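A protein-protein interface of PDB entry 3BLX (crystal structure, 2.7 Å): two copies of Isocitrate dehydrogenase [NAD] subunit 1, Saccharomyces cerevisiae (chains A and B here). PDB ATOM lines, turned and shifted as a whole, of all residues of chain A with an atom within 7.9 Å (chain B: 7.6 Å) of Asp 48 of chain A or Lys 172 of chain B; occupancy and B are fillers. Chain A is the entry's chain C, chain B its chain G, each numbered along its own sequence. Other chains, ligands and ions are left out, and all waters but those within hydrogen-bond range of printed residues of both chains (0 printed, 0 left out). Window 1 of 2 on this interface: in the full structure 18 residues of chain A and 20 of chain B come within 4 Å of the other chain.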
ATOM      1  N   LYS A  12      -0.597 -20.721  -6.120  1.00  0.00           N
ATOM      2  CA  LYS A  12      -0.807 -21.340  -4.823  1.00  0.00           C
ATOM      3  C   LYS A  12      -1.539 -22.658  -5.057  1.00  0.00           C
ATOM      4  O   LYS A  12      -2.585 -22.699  -5.710  1.00  0.00           O
ATOM      5  CB  LYS A  12      -1.621 -20.398  -3.919  1.00  0.00           C
ATOM      6  CG  LYS A  12      -1.825 -20.901  -2.508  1.00  0.00           C
ATOM      7  CD  LYS A  12      -2.653 -19.933  -1.645  1.00  0.00           C
ATOM      8  CE  LYS A  12      -1.941 -18.612  -1.438  1.00  0.00           C
ATOM      9  NZ  LYS A  12      -0.678 -18.676  -0.677  1.00  0.00           N
ATOM     10  N   TYR A  14      -2.298 -26.645  -3.232  1.00  0.00           N
ATOM     11  CA  TYR A  14      -2.184 -27.611  -2.150  1.00  0.00           C
ATOM     12  C   TYR A  14      -2.869 -28.876  -2.562  1.00  0.00           C
ATOM     13  O   TYR A  14      -4.032 -28.849  -3.008  1.00  0.00           O
ATOM     14  CB  TYR A  14      -2.799 -27.086  -0.858  1.00  0.00           C
ATOM     15  CG  TYR A  14      -2.058 -25.915  -0.301  1.00  0.00           C
ATOM     16  CD1 TYR A  14      -2.619 -24.662  -0.260  1.00  0.00           C
ATOM     17  CD2 TYR A  14      -0.766 -26.065   0.165  1.00  0.00           C
ATOM     18  CE1 TYR A  14      -1.899 -23.576   0.264  1.00  0.00           C
ATOM     19  CE2 TYR A  14      -0.052 -25.015   0.669  1.00  0.00           C
ATOM     20  CZ  TYR A  14      -0.610 -23.772   0.718  1.00  0.00           C
ATOM     21  OH  TYR A  14       0.136 -22.755   1.249  1.00  0.00           O
ATOM     22  N   ARG A  17      -4.961 -28.902  -5.548  1.00  0.00           N
ATOM     23  CA  ARG A  17      -5.969 -27.841  -5.726  1.00  0.00           C
ATOM     24  C   ARG A  17      -5.390 -26.442  -5.730  1.00  0.00           C
ATOM     25  O   ARG A  17      -4.639 -26.057  -4.838  1.00  0.00           O
ATOM     26  CB  ARG A  17      -7.049 -27.868  -4.652  1.00  0.00           C
ATOM     27  CG  ARG A  17      -7.611 -29.202  -4.311  1.00  0.00           C
ATOM     28  CD  ARG A  17      -8.908 -29.019  -3.527  1.00  0.00           C
ATOM     29  NE  ARG A  17      -9.987 -29.372  -4.426  1.00  0.00           N
ATOM     30  CZ  ARG A  17     -10.864 -28.513  -4.898  1.00  0.00           C
ATOM     31  NH1 ARG A  17     -10.807 -27.268  -4.504  1.00  0.00           N
ATOM     32  NH2 ARG A  17     -11.792 -28.910  -5.740  1.00  0.00           N
ATOM     33  N   PHE A  18      -5.813 -25.658  -6.704  1.00  0.00           N
ATOM     34  CA  PHE A  18      -5.386 -24.269  -6.815  1.00  0.00           C
ATOM     35  C   PHE A  18      -6.317 -23.308  -6.098  1.00  0.00           C
ATOM     36  O   PHE A  18      -7.538 -23.412  -6.238  1.00  0.00           O
ATOM     37  CB  PHE A  18      -5.389 -23.870  -8.271  1.00  0.00           C
ATOM     38  CG  PHE A  18      -4.452 -24.627  -9.103  1.00  0.00           C
ATOM     39  CD1 PHE A  18      -3.140 -24.197  -9.251  1.00  0.00           C
ATOM     40  CD2 PHE A  18      -4.869 -25.787  -9.758  1.00  0.00           C
ATOM     41  CE1 PHE A  18      -2.246 -24.916 -10.032  1.00  0.00           C
ATOM     42  CE2 PHE A  18      -3.987 -26.508 -10.547  1.00  0.00           C
ATOM     43  CZ  PHE A  18      -2.672 -26.068 -10.685  1.00  0.00           C
ATOM     44  N   THR A  19      -5.756 -22.354  -5.356  1.00  0.00           N
ATOM     45  CA  THR A  19      -6.553 -21.215  -4.882  1.00  0.00           C
ATOM     46  C   THR A  19      -6.406 -20.059  -5.864  1.00  0.00           C
ATOM     47  O   THR A  19      -5.308 -19.556  -6.022  1.00  0.00           O
ATOM     48  CB  THR A  19      -6.098 -20.731  -3.507  1.00  0.00           C
ATOM     49  OG1 THR A  19      -6.169 -21.821  -2.590  1.00  0.00           O
ATOM     50  CG2 THR A  19      -6.988 -19.603  -3.014  1.00  0.00           C
ATOM     51  N   VAL A  20      -7.485 -19.661  -6.536  1.00  0.00           N
ATOM     52  CA  VAL A  20      -7.410 -18.496  -7.407  1.00  0.00           C
ATOM     53  C   VAL A  20      -8.335 -17.352  -6.977  1.00  0.00           C
ATOM     54  O   VAL A  20      -9.461 -17.555  -6.596  1.00  0.00           O
ATOM     55  CB  VAL A  20      -7.560 -18.832  -8.927  1.00  0.00           C
ATOM     56  CG1 VAL A  20      -7.468 -20.323  -9.146  1.00  0.00           C
ATOM     57  CG2 VAL A  20      -8.811 -18.261  -9.492  1.00  0.00           C
ATOM     58  N   THR A  21      -7.812 -16.141  -7.043  1.00  0.00           N
ATOM     59  CA  THR A  21      -8.558 -14.927  -6.768  1.00  0.00           C
ATOM     60  C   THR A  21      -9.714 -14.736  -7.739  1.00  0.00           C
ATOM     61  O   THR A  21      -9.562 -14.891  -8.941  1.00  0.00           O
ATOM     62  CB  THR A  21      -7.635 -13.721  -6.820  1.00  0.00           C
ATOM     63  OG1 THR A  21      -6.598 -13.882  -5.845  1.00  0.00           O
ATOM     64  CG2 THR A  21      -8.408 -12.462  -6.510  1.00  0.00           C
ATOM     65  N   LEU A  22     -10.892 -14.465  -7.190  1.00  0.00           N
ATOM     66  CA  LEU A  22     -12.060 -14.191  -8.006  1.00  0.00           C
ATOM     67  C   LEU A  22     -12.596 -12.818  -7.651  1.00  0.00           C
ATOM     68  O   LEU A  22     -12.965 -12.596  -6.519  1.00  0.00           O
ATOM     69  CB  LEU A  22     -13.128 -15.220  -7.768  1.00  0.00           C
ATOM     70  CG  LEU A  22     -14.307 -15.120  -8.727  1.00  0.00           C
ATOM     71  CD1 LEU A  22     -13.837 -15.237 -10.146  1.00  0.00           C
ATOM     72  CD2 LEU A  22     -15.252 -16.204  -8.462  1.00  0.00           C
ATOM     73  N   PHE A  40     -17.744 -24.598 -13.594  1.00  0.00           N
ATOM     74  CA  PHE A  40     -16.561 -25.155 -12.955  1.00  0.00           C
ATOM     75  C   PHE A  40     -16.894 -26.224 -11.924  1.00  0.00           C
ATOM     76  O   PHE A  40     -16.225 -27.239 -11.874  1.00  0.00           O
ATOM     77  CB  PHE A  40     -15.682 -24.053 -12.339  1.00  0.00           C
ATOM     78  CG  PHE A  40     -14.617 -23.533 -13.268  1.00  0.00           C
ATOM     79  CD1 PHE A  40     -14.876 -23.381 -14.622  1.00  0.00           C
ATOM     80  CD2 PHE A  40     -13.375 -23.179 -12.790  1.00  0.00           C
ATOM     81  CE1 PHE A  40     -13.913 -22.894 -15.484  1.00  0.00           C
ATOM     82  CE2 PHE A  40     -12.410 -22.694 -13.646  1.00  0.00           C
ATOM     83  CZ  PHE A  40     -12.675 -22.555 -14.999  1.00  0.00           C
ATOM     84  N   ILE A  45     -13.754 -29.128 -11.134  1.00  0.00           N
ATOM     85  CA  ILE A  45     -12.381 -28.704 -11.345  1.00  0.00           C
ATOM     86  C   ILE A  45     -11.728 -28.380 -10.007  1.00  0.00           C
ATOM     87  O   ILE A  45     -12.370 -27.811  -9.121  1.00  0.00           O
ATOM     88  CB  ILE A  45     -12.329 -27.486 -12.309  1.00  0.00           C
ATOM     89  CG1 ILE A  45     -12.770 -27.901 -13.715  1.00  0.00           C
ATOM     90  CG2 ILE A  45     -10.929 -26.903 -12.380  1.00  0.00           C
ATOM     91  CD1 ILE A  45     -12.844 -26.764 -14.694  1.00  0.00           C
ATOM     92  N   PRO A  46     -10.451 -28.757  -9.846  1.00  0.00           N
ATOM     93  CA  PRO A  46      -9.730 -28.578  -8.585  1.00  0.00           C
ATOM     94  C   PRO A  46      -9.345 -27.123  -8.334  1.00  0.00           C
ATOM     95  O   PRO A  46      -8.178 -26.816  -8.169  1.00  0.00           O
ATOM     96  CB  PRO A  46      -8.459 -29.406  -8.776  1.00  0.00           C
ATOM     97  CG  PRO A  46      -8.544 -30.011 -10.115  1.00  0.00           C
ATOM     98  CD  PRO A  46      -9.593 -29.325 -10.890  1.00  0.00           C
ATOM     99  N   ILE A  47     -10.329 -26.239  -8.313  1.00  0.00           N
ATOM    100  CA  ILE A  47     -10.083 -24.841  -8.077  1.00  0.00           C
ATOM    101  C   ILE A  47     -10.967 -24.353  -6.950  1.00  0.00           C
ATOM    102  O   ILE A  47     -12.184 -24.509  -6.981  1.00  0.00           O
ATOM    103  CB  ILE A  47     -10.294 -24.009  -9.361  1.00  0.00           C
ATOM    104  CG1 ILE A  47      -9.194 -24.312 -10.348  1.00  0.00           C
ATOM    105  CG2 ILE A  47     -10.305 -22.495  -9.063  1.00  0.00           C
ATOM    106  CD1 ILE A  47      -9.295 -23.557 -11.621  1.00  0.00           C
ATOM    107  N   ASP A  48     -10.336 -23.770  -5.944  1.00  0.00           N
ATOM    108  CA  ASP A  48     -11.038 -23.053  -4.903  1.00  0.00           C
ATOM    109  C   ASP A  48     -10.966 -21.538  -5.129  1.00  0.00           C
ATOM    110  O   ASP A  48      -9.884 -20.955  -5.183  1.00  0.00           O
ATOM    111  CB  ASP A  48     -10.420 -23.397  -3.542  1.00  0.00           C
ATOM    112  CG  ASP A  48     -10.651 -24.849  -3.133  1.00  0.00           C
ATOM    113  OD1 ASP A  48     -11.667 -25.462  -3.555  1.00  0.00           O
ATOM    114  OD2 ASP A  48      -9.815 -25.362  -2.353  1.00  0.00           O
ATOM    115  N   TRP A  49     -12.120 -20.904  -5.242  1.00  0.00           N
ATOM    116  CA  TRP A  49     -12.159 -19.456  -5.378  1.00  0.00           C
ATOM    117  C   TRP A  49     -11.898 -18.756  -4.057  1.00  0.00           C
ATOM    118  O   TRP A  49     -12.454 -19.123  -3.032  1.00  0.00           O
ATOM    119  CB  TRP A  49     -13.497 -19.039  -5.925  1.00  0.00           C
ATOM    120  CG  TRP A  49     -13.892 -19.788  -7.139  1.00  0.00           C
ATOM    121  CD1 TRP A  49     -14.873 -20.724  -7.239  1.00  0.00           C
ATOM    122  CD2 TRP A  49     -13.324 -19.659  -8.439  1.00  0.00           C
ATOM    123  NE1 TRP A  49     -14.951 -21.185  -8.517  1.00  0.00           N
ATOM    124  CE2 TRP A  49     -14.007 -20.546  -9.282  1.00  0.00           C
ATOM    125  CE3 TRP A  49     -12.303 -18.877  -8.976  1.00  0.00           C
ATOM    126  CZ2 TRP A  49     -13.704 -20.673 -10.635  1.00  0.00           C
ATOM    127  CZ3 TRP A  49     -12.013 -19.002 -10.318  1.00  0.00           C
ATOM    128  CH2 TRP A  49     -12.715 -19.891 -11.132  1.00  0.00           C
ATOM    129  N   GLU A  50     -11.031 -17.760  -4.076  1.00  0.00           N
ATOM    130  CA  GLU A  50     -10.925 -16.839  -2.966  1.00  0.00           C
ATOM    131  C   GLU A  50     -11.590 -15.564  -3.451  1.00  0.00           C
ATOM    132  O   GLU A  50     -10.945 -14.710  -4.031  1.00  0.00           O
ATOM    133  CB  GLU A  50      -9.469 -16.583  -2.601  1.00  0.00           C
ATOM    134  CG  GLU A  50      -9.247 -15.631  -1.421  1.00  0.00           C
ATOM    135  CD  GLU A  50      -7.783 -15.515  -1.007  1.00  0.00           C
ATOM    136  OE1 GLU A  50      -7.378 -14.466  -0.483  1.00  0.00           O
ATOM    137  OE2 GLU A  50      -7.019 -16.469  -1.205  1.00  0.00           O
ATOM    138  N   THR A  51     -12.895 -15.467  -3.244  1.00  0.00           N
ATOM    139  CA  THR A  51     -13.662 -14.403  -3.836  1.00  0.00           C
ATOM    140  C   THR A  51     -13.566 -13.075  -3.048  1.00  0.00           C
ATOM    141  O   THR A  51     -13.716 -13.041  -1.838  1.00  0.00           O
ATOM    142  CB  THR A  51     -15.101 -14.867  -4.157  1.00  0.00           C
ATOM    143  OG1 THR A  51     -15.994 -13.754  -4.066  1.00  0.00           O
ATOM    144  CG2 THR A  51     -15.542 -15.965  -3.234  1.00  0.00           C
ATOM    145  N   ASN A  73      -1.981 -15.608  -4.264  1.00  0.00           N
ATOM    146  CA  ASN A  73      -2.410 -16.646  -5.172  1.00  0.00           C
ATOM    147  C   ASN A  73      -1.731 -16.613  -6.530  1.00  0.00           C
ATOM    148  O   ASN A  73      -1.624 -17.634  -7.191  1.00  0.00           O
ATOM    149  CB  ASN A  73      -3.934 -16.636  -5.342  1.00  0.00           C
ATOM    150  CG  ASN A  73      -4.679 -16.737  -4.026  1.00  0.00           C
ATOM    151  OD1 ASN A  73      -4.156 -17.217  -3.030  1.00  0.00           O
ATOM    152  ND2 ASN A  73      -5.915 -16.281  -4.023  1.00  0.00           N
ATOM    153  N   ALA B 166      -0.141 -23.009   6.992  1.00  0.00           N
ATOM    154  CA  ALA B 166      -0.945 -22.882   8.196  1.00  0.00           C
ATOM    155  C   ALA B 166      -1.941 -21.732   8.089  1.00  0.00           C
ATOM    156  O   ALA B 166      -3.108 -21.879   8.426  1.00  0.00           O
ATOM    157  CB  ALA B 166      -0.056 -22.706   9.408  1.00  0.00           C
ATOM    158  N   PHE B 167      -1.474 -20.589   7.605  1.00  0.00           N
ATOM    159  CA  PHE B 167      -2.339 -19.428   7.462  1.00  0.00           C
ATOM    160  C   PHE B 167      -3.379 -19.642   6.383  1.00  0.00           C
ATOM    161  O   PHE B 167      -4.536 -19.282   6.569  1.00  0.00           O
ATOM    162  CB  PHE B 167      -1.539 -18.175   7.188  1.00  0.00           C
ATOM    163  CG  PHE B 167      -0.792 -17.682   8.370  1.00  0.00           C
ATOM    164  CD1 PHE B 167      -1.463 -17.288   9.492  1.00  0.00           C
ATOM    165  CD2 PHE B 167       0.583 -17.595   8.354  1.00  0.00           C
ATOM    166  CE1 PHE B 167      -0.800 -16.837  10.574  1.00  0.00           C
ATOM    167  CE2 PHE B 167       1.262 -17.136   9.439  1.00  0.00           C
ATOM    168  CZ  PHE B 167       0.570 -16.750  10.558  1.00  0.00           C
ATOM    169  N   ASP B 168      -2.980 -20.267   5.278  1.00  0.00           N
ATOM    170  CA  ASP B 168      -3.923 -20.590   4.215  1.00  0.00           C
ATOM    171  C   ASP B 168      -5.020 -21.507   4.678  1.00  0.00           C
ATOM    172  O   ASP B 168      -6.136 -21.436   4.181  1.00  0.00           O
ATOM    173  CB  ASP B 168      -3.213 -21.173   3.003  1.00  0.00           C
ATOM    174  CG  ASP B 168      -2.521 -20.093   2.151  1.00  0.00           C
ATOM    175  OD1 ASP B 168      -2.981 -18.909   2.143  1.00  0.00           O
ATOM    176  OD2 ASP B 168      -1.517 -20.442   1.492  1.00  0.00           O
ATOM    177  N   PHE B 169      -4.689 -22.321   5.679  1.00  0.00           N
ATOM    178  CA  PHE B 169      -5.579 -23.334   6.228  1.00  0.00           C
ATOM    179  C   PHE B 169      -6.529 -22.686   7.210  1.00  0.00           C
ATOM    180  O   PHE B 169      -7.743 -22.919   7.170  1.00  0.00           O
ATOM    181  CB  PHE B 169      -4.744 -24.412   6.906  1.00  0.00           C
ATOM    182  CG  PHE B 169      -5.494 -25.641   7.263  1.00  0.00           C
ATOM    183  CD1 PHE B 169      -6.125 -25.749   8.495  1.00  0.00           C
ATOM    184  CD2 PHE B 169      -5.528 -26.709   6.393  1.00  0.00           C
ATOM    185  CE1 PHE B 169      -6.800 -26.898   8.839  1.00  0.00           C
ATOM    186  CE2 PHE B 169      -6.200 -27.876   6.734  1.00  0.00           C
ATOM    187  CZ  PHE B 169      -6.832 -27.973   7.957  1.00  0.00           C
ATOM    188  N   ALA B 170      -5.981 -21.849   8.079  1.00  0.00           N
ATOM    189  CA  ALA B 170      -6.818 -21.015   8.927  1.00  0.00           C
ATOM    190  C   ALA B 170      -7.867 -20.210   8.124  1.00  0.00           C
ATOM    191  O   ALA B 170      -9.044 -20.230   8.459  1.00  0.00           O
ATOM    192  CB  ALA B 170      -5.966 -20.112   9.768  1.00  0.00           C
ATOM    193  N   LYS B 171      -7.432 -19.531   7.062  1.00  0.00           N
ATOM    194  CA  LYS B 171      -8.313 -18.778   6.173  1.00  0.00           C
ATOM    195  C   LYS B 171      -9.433 -19.652   5.619  1.00  0.00           C
ATOM    196  O   LYS B 171     -10.590 -19.308   5.703  1.00  0.00           O
ATOM    197  CB  LYS B 171      -7.512 -18.221   5.008  1.00  0.00           C
ATOM    198  CG  LYS B 171      -7.946 -16.877   4.435  1.00  0.00           C
ATOM    199  CD  LYS B 171      -7.270 -15.753   5.190  1.00  0.00           C
ATOM    200  CE  LYS B 171      -7.613 -14.352   4.666  1.00  0.00           C
ATOM    201  NZ  LYS B 171      -7.079 -13.267   5.584  1.00  0.00           N
ATOM    202  N   LYS B 172      -9.080 -20.787   5.042  1.00  0.00           N
ATOM    203  CA  LYS B 172     -10.045 -21.657   4.395  1.00  0.00           C
ATOM    204  C   LYS B 172     -11.086 -22.255   5.362  1.00  0.00           C
ATOM    205  O   LYS B 172     -12.234 -22.470   4.993  1.00  0.00           O
ATOM    206  CB  LYS B 172      -9.302 -22.779   3.653  1.00  0.00           C
ATOM    207  CG  LYS B 172     -10.112 -23.497   2.583  1.00  0.00           C
ATOM    208  CD  LYS B 172      -9.493 -24.824   2.194  1.00  0.00           C
ATOM    209  CE  LYS B 172     -10.069 -25.345   0.893  1.00  0.00           C
ATOM    210  NZ  LYS B 172      -9.605 -26.747   0.639  1.00  0.00           N
ATOM    211  N   TYR B 173     -10.685 -22.531   6.597  1.00  0.00           N
ATOM    212  CA  TYR B 173     -11.597 -23.179   7.526  1.00  0.00           C
ATOM    213  C   TYR B 173     -12.033 -22.229   8.626  1.00  0.00           C
ATOM    214  O   TYR B 173     -12.484 -22.665   9.682  1.00  0.00           O
ATOM    215  CB  TYR B 173     -11.010 -24.495   8.078  1.00  0.00           C
ATOM    216  CG  TYR B 173     -10.799 -25.518   6.986  1.00  0.00           C
ATOM    217  CD1 TYR B 173      -9.526 -25.777   6.488  1.00  0.00           C
ATOM    218  CD2 TYR B 173     -11.875 -26.194   6.417  1.00  0.00           C
ATOM    219  CE1 TYR B 173      -9.330 -26.690   5.469  1.00  0.00           C
ATOM    220  CE2 TYR B 173     -11.678 -27.112   5.403  1.00  0.00           C
ATOM    221  CZ  TYR B 173     -10.408 -27.355   4.939  1.00  0.00           C
ATOM    222  OH  TYR B 173     -10.218 -28.262   3.934  1.00  0.00           O
ATOM    223  N   ASN B 174     -11.905 -20.933   8.362  1.00  0.00           N
ATOM    224  CA  ASN B 174     -12.373 -19.889   9.274  1.00  0.00           C
ATOM    225  C   ASN B 174     -11.890 -20.062  10.702  1.00  0.00           C
ATOM    226  O   ASN B 174     -12.662 -19.992  11.641  1.00  0.00           O
ATOM    227  CB  ASN B 174     -13.893 -19.756   9.233  1.00  0.00           C
ATOM    228  CG  ASN B 174     -14.373 -19.090   7.969  1.00  0.00           C
ATOM    229  OD1 ASN B 174     -14.347 -17.856   7.856  1.00  0.00           O
ATOM    230  ND2 ASN B 174     -14.810 -19.901   7.000  1.00  0.00           N
ATOM    231  N   ARG B 175     -10.597 -20.298  10.841  1.00  0.00           N
ATOM    232  CA  ARG B 175      -9.966 -20.290  12.126  1.00  0.00           C
ATOM    233  C   ARG B 175      -9.414 -18.888  12.344  1.00  0.00           C
ATOM    234  O   ARG B 175      -9.071 -18.205  11.392  1.00  0.00           O
ATOM    235  CB  ARG B 175      -8.872 -21.351  12.165  1.00  0.00           C
ATOM    236  CG  ARG B 175      -9.296 -22.664  12.804  1.00  0.00           C
ATOM    237  CD  ARG B 175     -10.434 -23.286  12.069  1.00  0.00           C
ATOM    238  NE  ARG B 175     -10.941 -24.516  12.694  1.00  0.00           N
ATOM    239  CZ  ARG B 175     -10.650 -24.973  13.918  1.00  0.00           C
ATOM    240  NH1 ARG B 175      -9.836 -24.317  14.729  1.00  0.00           N
ATOM    241  NH2 ARG B 175     -11.194 -26.111  14.334  1.00  0.00           N
ATOM    242  N   ILE B 209      -5.866 -12.584  10.636  1.00  0.00           N
ATOM    243  CA  ILE B 209      -5.606 -13.705  11.518  1.00  0.00           C
ATOM    244  C   ILE B 209      -4.659 -13.327  12.655  1.00  0.00           C
ATOM    245  O   ILE B 209      -3.629 -12.699  12.441  1.00  0.00           O
ATOM    246  CB  ILE B 209      -5.081 -14.922  10.726  1.00  0.00           C
ATOM    247  CG1 ILE B 209      -6.184 -15.438   9.808  1.00  0.00           C
ATOM    248  CG2 ILE B 209      -4.627 -16.031  11.663  1.00  0.00           C
ATOM    249  CD1 ILE B 209      -5.751 -16.511   8.894  1.00  0.00           C
ATOM    250  N   PHE B 262      -0.004 -33.036   3.226  1.00  0.00           N
ATOM    251  CA  PHE B 262      -0.042 -32.306   1.961  1.00  0.00           C
ATOM    252  C   PHE B 262       1.319 -31.953   1.453  1.00  0.00           C
ATOM    253  O   PHE B 262       2.207 -31.584   2.219  1.00  0.00           O
ATOM    254  CB  PHE B 262      -0.841 -31.001   2.090  1.00  0.00           C
ATOM    255  CG  PHE B 262      -2.292 -31.204   2.417  1.00  0.00           C
ATOM    256  CD1 PHE B 262      -2.716 -31.235   3.721  1.00  0.00           C
ATOM    257  CD2 PHE B 262      -3.223 -31.336   1.422  1.00  0.00           C
ATOM    258  CE1 PHE B 262      -4.031 -31.402   4.026  1.00  0.00           C
ATOM    259  CE2 PHE B 262      -4.548 -31.516   1.726  1.00  0.00           C
ATOM    260  CZ  PHE B 262      -4.950 -31.559   3.032  1.00  0.00           C
ATOM    261  N   ASN B 300     -13.793 -34.131   0.751  1.00  0.00           N
ATOM    262  CA  ASN B 300     -13.760 -32.693   0.639  1.00  0.00           C
ATOM    263  C   ASN B 300     -12.746 -32.274  -0.411  1.00  0.00           C
ATOM    264  O   ASN B 300     -13.050 -31.538  -1.329  1.00  0.00           O
ATOM    265  CB  ASN B 300     -13.398 -32.061   1.976  1.00  0.00           C
ATOM    266  CG  ASN B 300     -14.555 -32.059   2.945  1.00  0.00           C
ATOM    267  OD1 ASN B 300     -15.682 -32.297   2.548  1.00  0.00           O
ATOM    268  ND2 ASN B 300     -14.282 -31.774   4.222  1.00  0.00           N
ATOM    269  N   HIS B 301     -11.540 -32.787  -0.286  1.00  0.00           N
ATOM    270  CA  HIS B 301     -10.464 -32.382  -1.155  1.00  0.00           C
ATOM    271  C   HIS B 301     -10.756 -32.732  -2.603  1.00  0.00           C
ATOM    272  O   HIS B 301     -10.388 -32.006  -3.517  1.00  0.00           O
ATOM    273  CB  HIS B 301      -9.174 -33.063  -0.715  1.00  0.00           C
ATOM    274  CG  HIS B 301      -7.947 -32.418  -1.263  1.00  0.00           C
ATOM    275  ND1 HIS B 301      -7.268 -32.919  -2.358  1.00  0.00           N
ATOM    276  CD2 HIS B 301      -7.281 -31.303  -0.880  1.00  0.00           C
ATOM    277  CE1 HIS B 301      -6.219 -32.154  -2.605  1.00  0.00           C
ATOM    278  NE2 HIS B 301      -6.201 -31.175  -1.723  1.00  0.00           N
ATOM    279  N   GLY B 303     -13.497 -32.720  -4.015  1.00  0.00           N
ATOM    280  CA  GLY B 303     -14.622 -31.947  -4.496  1.00  0.00           C
ATOM    281  C   GLY B 303     -15.967 -32.632  -4.360  1.00  0.00           C
ATOM    282  O   GLY B 303     -17.007 -32.039  -4.682  1.00  0.00           O
ATOM    283  N   ASN B 305     -17.803 -34.432  -1.204  1.00  0.00           N
ATOM    284  CA  ASN B 305     -18.123 -33.653   0.021  1.00  0.00           C
ATOM    285  C   ASN B 305     -19.613 -33.395   0.341  1.00  0.00           C
ATOM    286  O   ASN B 305     -19.970 -33.003   1.456  1.00  0.00           O
ATOM    287  CB  ASN B 305     -17.217 -32.380   0.188  1.00  0.00           C
ATOM    288  CG  ASN B 305     -17.750 -31.139  -0.528  1.00  0.00           C
ATOM    289  OD1 ASN B 305     -18.954 -30.902  -0.569  1.00  0.00           O
ATOM    290  ND2 ASN B 305     -16.838 -30.330  -1.082  1.00  0.00           N
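Asp 48 of chain A touches just one residue of chain B: Lys 172 (3.3 Å). Lys 172 of chain B touches just one residue of chain A: Asp 48. Printed residues of chain A within 4 Å of Asp 168 of chain B: Lys 12 (2.9 Å) and Tyr 14 (2.9 Å). Of the printed residues of chain B, Tyr 14 of chain A touches Asp 168 and His 301.
OH of Tyr 14 of chain A is in hydrogen-bond range of OD2 of Asp 168 of chain B (2.9 Å). A ring nitrogen (NE2) of His 301 of chain B is in hydrogen-bond range of the backbone carbonyl oxygen (O) of Tyr 14 of chain A, 3.4 Å away. The side-chain amino group of Lys 172 of chain B lies within salt-bridge range of the side-chain carboxylate of Asp 48 of chain A, at 3.3 Å. The side-chain carboxylate of Asp 168 of chain B lies within salt-bridge range of the side-chain amino group of Lys 12 of chain A, 2.9 Å away. NE of Arg 17 of chain A is in hydrogen-bond range of O of His 301 of chain B, 2.8 Å away.
Of the 16 printed residues of chain B, 3 touch a printed residue of chain A. Hydrophobic or aromatic side chains of chain B within 4 Å of the printed part of chain A: His 301. Along chain B the printed residues that touch a printed residue of chain A span positions 168 to 301. Of the 17 printed residues of chain A, 4 touch a printed residue of chain B.
No position is printed for both chains. Of the 5 pairs that touch across the chains among the printed residues, none has its exchanged pair printed and touching as well.
The backbone carbonyl oxygen (O) of Phe 18 of chain A is in hydrogen-bond range of the backbone NH (N) of Asp 48 of chain A, 2.8 Å away. The backbone NH (N) of Val 20 of chain A sits at hydrogen-bond distance from the backbone carbonyl oxygen (O) of Asp 48 of chain A, at 3.0 Å. NH1 of Arg 17 of chain A is in salt-bridge range of OD2 of Asp 48 of chain A, 3.0 Å away. The backbone NH of Lys 12 of chain A lies within hydrogen-bond range of the backbone carbonyl oxygen of Asn 73 of chain A (3.4 Å). O of Lys 12 of chain A sits at hydrogen-bond distance from N of Thr 19 of chain A (3.2 Å).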
